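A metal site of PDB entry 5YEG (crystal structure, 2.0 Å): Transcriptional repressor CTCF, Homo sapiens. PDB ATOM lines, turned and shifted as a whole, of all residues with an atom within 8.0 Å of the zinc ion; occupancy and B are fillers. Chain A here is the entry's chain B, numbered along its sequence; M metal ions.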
ATOM      1  N   LYS A 120      16.164  34.716 -22.745  1.00  0.00           N
ATOM      2  CA  LYS A 120      16.411  33.285 -22.922  1.00  0.00           C
ATOM      3  C   LYS A 120      15.486  32.707 -23.984  1.00  0.00           C
ATOM      4  O   LYS A 120      14.295  33.051 -24.043  1.00  0.00           O
ATOM      5  CB  LYS A 120      16.200  32.536 -21.599  1.00  0.00           C
ATOM      6  CG  LYS A 120      16.664  31.092 -21.630  1.00  0.00           C
ATOM      7  CD  LYS A 120      16.316  30.320 -20.342  1.00  0.00           C
ATOM      8  CE  LYS A 120      14.879  29.788 -20.359  1.00  0.00           C
ATOM      9  NZ  LYS A 120      14.678  28.750 -21.434  1.00  0.00           N
ATOM     10  N   CYS A 121      16.024  31.826 -24.815  1.00  0.00           N
ATOM     11  CA  CYS A 121      15.203  31.053 -25.742  1.00  0.00           C
ATOM     12  C   CYS A 121      14.075  30.379 -24.985  1.00  0.00           C
ATOM     13  O   CYS A 121      14.263  29.880 -23.868  1.00  0.00           O
ATOM     14  CB  CYS A 121      16.073  30.009 -26.460  1.00  0.00           C
ATOM     15  SG  CYS A 121      15.231  28.810 -27.577  1.00  0.00           S
ATOM     16  N   ARG A 122      12.891  30.371 -25.573  1.00  0.00           N
ATOM     17  CA  ARG A 122      11.774  29.709 -24.896  1.00  0.00           C
ATOM     18  C   ARG A 122      11.869  28.191 -24.934  1.00  0.00           C
ATOM     19  O   ARG A 122      11.108  27.525 -24.232  1.00  0.00           O
ATOM     20  CB  ARG A 122      10.449  30.175 -25.514  1.00  0.00           C
ATOM     21  CG  ARG A 122      10.326  29.883 -27.005  1.00  0.00           C
ATOM     22  CD  ARG A 122       9.040  30.436 -27.628  1.00  0.00           C
ATOM     23  NE  ARG A 122       7.834  29.755 -27.148  1.00  0.00           N
ATOM     24  CZ  ARG A 122       6.671  29.741 -27.799  1.00  0.00           C
ATOM     25  NH1 ARG A 122       6.551  30.360 -28.959  1.00  0.00           N
ATOM     26  NH2 ARG A 122       5.644  29.081 -27.291  1.00  0.00           N
ATOM     27  N   TYR A 123      12.821  27.622 -25.678  1.00  0.00           N
ATOM     28  CA  TYR A 123      12.943  26.170 -25.787  1.00  0.00           C
ATOM     29  C   TYR A 123      14.257  25.598 -25.284  1.00  0.00           C
ATOM     30  O   TYR A 123      14.374  24.375 -25.195  1.00  0.00           O
ATOM     31  CB  TYR A 123      12.734  25.717 -27.240  1.00  0.00           C
ATOM     32  CG  TYR A 123      11.516  26.309 -27.888  1.00  0.00           C
ATOM     33  CD1 TYR A 123      10.258  26.188 -27.294  1.00  0.00           C
ATOM     34  CD2 TYR A 123      11.605  26.978 -29.095  1.00  0.00           C
ATOM     35  CE1 TYR A 123       9.135  26.733 -27.884  1.00  0.00           C
ATOM     36  CE2 TYR A 123      10.487  27.520 -29.693  1.00  0.00           C
ATOM     37  CZ  TYR A 123       9.259  27.396 -29.088  1.00  0.00           C
ATOM     38  OH  TYR A 123       8.149  27.942 -29.696  1.00  0.00           O
ATOM     39  N   CYS A 124      15.258  26.438 -25.030  1.00  0.00           N
ATOM     40  CA  CYS A 124      16.552  25.960 -24.554  1.00  0.00           C
ATOM     41  C   CYS A 124      17.140  27.041 -23.662  1.00  0.00           C
ATOM     42  O   CYS A 124      16.537  28.094 -23.448  1.00  0.00           O
ATOM     43  CB  CYS A 124      17.454  25.531 -25.719  1.00  0.00           C
ATOM     44  SG  CYS A 124      18.370  26.816 -26.568  1.00  0.00           S
ATOM     45  N   ASP A 125      18.295  26.761 -23.073  1.00  0.00           N
ATOM     46  CA  ASP A 125      18.884  27.698 -22.127  1.00  0.00           C
ATOM     47  C   ASP A 125      19.772  28.744 -22.780  1.00  0.00           C
ATOM     48  O   ASP A 125      20.495  29.450 -22.070  1.00  0.00           O
ATOM     49  CB  ASP A 125      19.634  26.928 -21.033  1.00  0.00           C
ATOM     50  CG  ASP A 125      20.821  26.136 -21.567  1.00  0.00           C
ATOM     51  OD1 ASP A 125      21.110  26.215 -22.784  1.00  0.00           O
ATOM     52  OD2 ASP A 125      21.446  25.403 -20.756  1.00  0.00           O
ATOM     53  N   ALA A 126      19.714  28.882 -24.104  1.00  0.00           N
ATOM     54  CA  ALA A 126      20.505  29.902 -24.776  1.00  0.00           C
ATOM     55  C   ALA A 126      19.927  31.291 -24.526  1.00  0.00           C
ATOM     56  O   ALA A 126      18.707  31.474 -24.475  1.00  0.00           O
ATOM     57  CB  ALA A 126      20.564  29.627 -26.275  1.00  0.00           C
ATOM     58  N   VAL A 127      20.817  32.271 -24.381  1.00  0.00           N
ATOM     59  CA  VAL A 127      20.438  33.641 -24.077  1.00  0.00           C
ATOM     60  C   VAL A 127      20.933  34.563 -25.184  1.00  0.00           C
ATOM     61  O   VAL A 127      22.020  34.358 -25.739  1.00  0.00           O
ATOM     62  CB  VAL A 127      21.010  34.071 -22.706  1.00  0.00           C
ATOM     63  CG1 VAL A 127      20.696  35.542 -22.409  1.00  0.00           C
ATOM     64  CG2 VAL A 127      20.427  33.200 -21.668  1.00  0.00           C
ATOM     65  N   PHE A 128      20.131  35.578 -25.502  1.00  0.00           N
ATOM     66  CA  PHE A 128      20.451  36.519 -26.561  1.00  0.00           C
ATOM     67  C   PHE A 128      20.227  37.927 -26.048  1.00  0.00           C
ATOM     68  O   PHE A 128      19.525  38.153 -25.058  1.00  0.00           O
ATOM     69  CB  PHE A 128      19.616  36.241 -27.819  1.00  0.00           C
ATOM     70  CG  PHE A 128      19.825  34.869 -28.363  1.00  0.00           C
ATOM     71  CD1 PHE A 128      19.152  33.785 -27.812  1.00  0.00           C
ATOM     72  CD2 PHE A 128      20.749  34.648 -29.366  1.00  0.00           C
ATOM     73  CE1 PHE A 128      19.373  32.510 -28.291  1.00  0.00           C
ATOM     74  CE2 PHE A 128      20.969  33.374 -29.845  1.00  0.00           C
ATOM     75  CZ  PHE A 128      20.286  32.303 -29.297  1.00  0.00           C
ATOM     76  N   LEU A 134      17.399  36.414 -31.250  1.00  0.00           N
ATOM     77  CA  LEU A 134      16.548  35.532 -30.453  1.00  0.00           C
ATOM     78  C   LEU A 134      15.557  34.773 -31.339  1.00  0.00           C
ATOM     79  O   LEU A 134      15.498  33.543 -31.298  1.00  0.00           O
ATOM     80  CB  LEU A 134      15.814  36.351 -29.392  1.00  0.00           C
ATOM     81  CG  LEU A 134      14.771  35.528 -28.625  1.00  0.00           C
ATOM     82  CD1 LEU A 134      15.462  34.430 -27.806  1.00  0.00           C
ATOM     83  CD2 LEU A 134      13.941  36.422 -27.722  1.00  0.00           C
ATOM     84  N   HIS A 137      17.137  32.242 -33.726  1.00  0.00           N
ATOM     85  CA  HIS A 137      17.530  31.039 -33.008  1.00  0.00           C
ATOM     86  C   HIS A 137      16.322  30.187 -32.668  1.00  0.00           C
ATOM     87  O   HIS A 137      16.347  28.956 -32.839  1.00  0.00           O
ATOM     88  CB  HIS A 137      18.280  31.376 -31.738  1.00  0.00           C
ATOM     89  CG  HIS A 137      18.437  30.191 -30.838  1.00  0.00           C
ATOM     90  ND1 HIS A 137      19.485  29.299 -30.967  1.00  0.00           N
ATOM     91  CD2 HIS A 137      17.661  29.715 -29.840  1.00  0.00           C
ATOM     92  CE1 HIS A 137      19.351  28.338 -30.072  1.00  0.00           C
ATOM     93  NE2 HIS A 137      18.254  28.567 -29.372  1.00  0.00           N
ATOM     94  N   GLN A 138      15.254  30.810 -32.155  1.00  0.00           N
ATOM     95  CA  GLN A 138      14.058  30.043 -31.785  1.00  0.00           C
ATOM     96  C   GLN A 138      13.475  29.309 -32.979  1.00  0.00           C
ATOM     97  O   GLN A 138      12.895  28.232 -32.818  1.00  0.00           O
ATOM     98  CB  GLN A 138      13.020  30.960 -31.138  1.00  0.00           C
ATOM     99  CG  GLN A 138      13.326  31.261 -29.677  1.00  0.00           C
ATOM    100  CD  GLN A 138      12.283  32.123 -29.003  1.00  0.00           C
ATOM    101  OE1 GLN A 138      12.320  32.305 -27.779  1.00  0.00           O
ATOM    102  NE2 GLN A 138      11.366  32.678 -29.785  1.00  0.00           N
ATOM    103  N   LYS A 139      13.623  29.851 -34.193  1.00  0.00           N
ATOM    104  CA  LYS A 139      13.120  29.124 -35.344  1.00  0.00           C
ATOM    105  C   LYS A 139      13.914  27.862 -35.638  1.00  0.00           C
ATOM    106  O   LYS A 139      13.431  26.997 -36.378  1.00  0.00           O
ATOM    107  CB  LYS A 139      13.110  30.027 -36.579  1.00  0.00           C
ATOM    108  CG  LYS A 139      12.000  31.071 -36.556  1.00  0.00           C
ATOM    109  CD  LYS A 139      12.271  32.165 -37.587  1.00  0.00           C
ATOM    110  CE  LYS A 139      11.095  32.358 -38.544  1.00  0.00           C
ATOM    111  NZ  LYS A 139      11.476  33.254 -39.682  1.00  0.00           N
ATOM    112  N   SER A 140      15.103  27.704 -35.050  1.00  0.00           N
ATOM    113  CA  SER A 140      15.934  26.527 -35.295  1.00  0.00           C
ATOM    114  C   SER A 140      15.486  25.300 -34.506  1.00  0.00           C
ATOM    115  O   SER A 140      16.071  24.223 -34.678  1.00  0.00           O
ATOM    116  CB  SER A 140      17.401  26.835 -34.977  1.00  0.00           C
ATOM    117  OG  SER A 140      17.664  26.669 -33.591  1.00  0.00           O
ATOM    118  N   HIS A 141      14.476  25.422 -33.651  1.00  0.00           N
ATOM    119  CA  HIS A 141      14.003  24.270 -32.881  1.00  0.00           C
ATOM    120  C   HIS A 141      12.975  23.454 -33.681  1.00  0.00           C
ATOM    121  O   HIS A 141      11.841  23.893 -33.887  1.00  0.00           O
ATOM    122  CB  HIS A 141      13.429  24.727 -31.536  1.00  0.00           C
ATOM    123  CG  HIS A 141      14.480  25.119 -30.535  1.00  0.00           C
ATOM    124  ND1 HIS A 141      15.017  24.232 -29.636  1.00  0.00           N
ATOM    125  CD2 HIS A 141      15.090  26.309 -30.308  1.00  0.00           C
ATOM    126  CE1 HIS A 141      15.917  24.851 -28.892  1.00  0.00           C
ATOM    127  NE2 HIS A 141      15.985  26.116 -29.277  1.00  0.00           N
HETATM  128 ZN    ZN M   1      16.844  27.438 -28.023  1.00  0.00          ZN
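The zinc ion is bound by NE2 of His 141 (2.0 Å).
SG of Cys 121 is bound to the zinc ion (2.2 Å).
SG of Cys 124 binds the zinc ion (2.2 Å).
NE2 of His 137 is bound to the zinc ion, at 2.3 Å.
The zinc ion has four donor atoms within binding distance.
SG of Cys 121 sits close to N of Tyr 123 (3.3 Å).
The backbone carbonyl oxygen of Ala 126 sits at hydrogen-bond distance from the backbone NH of Cys 121 (2.7 Å).
The side-chain sulfur (SG) of Cys 124 sits close to the backbone NH (N) of Ala 126, 3.5 Å away.
The backbone carbonyl oxygen of Cys 124 is in hydrogen-bond range of the side-chain amino group of Lys 120 (2.8 Å).
O of His 137 sits at hydrogen-bond distance from OG of Ser 140 (2.7 Å).
Four residues have an atom within 4 Å of the zinc ion: Cys 121, Cys 124, His 137 and His 141.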
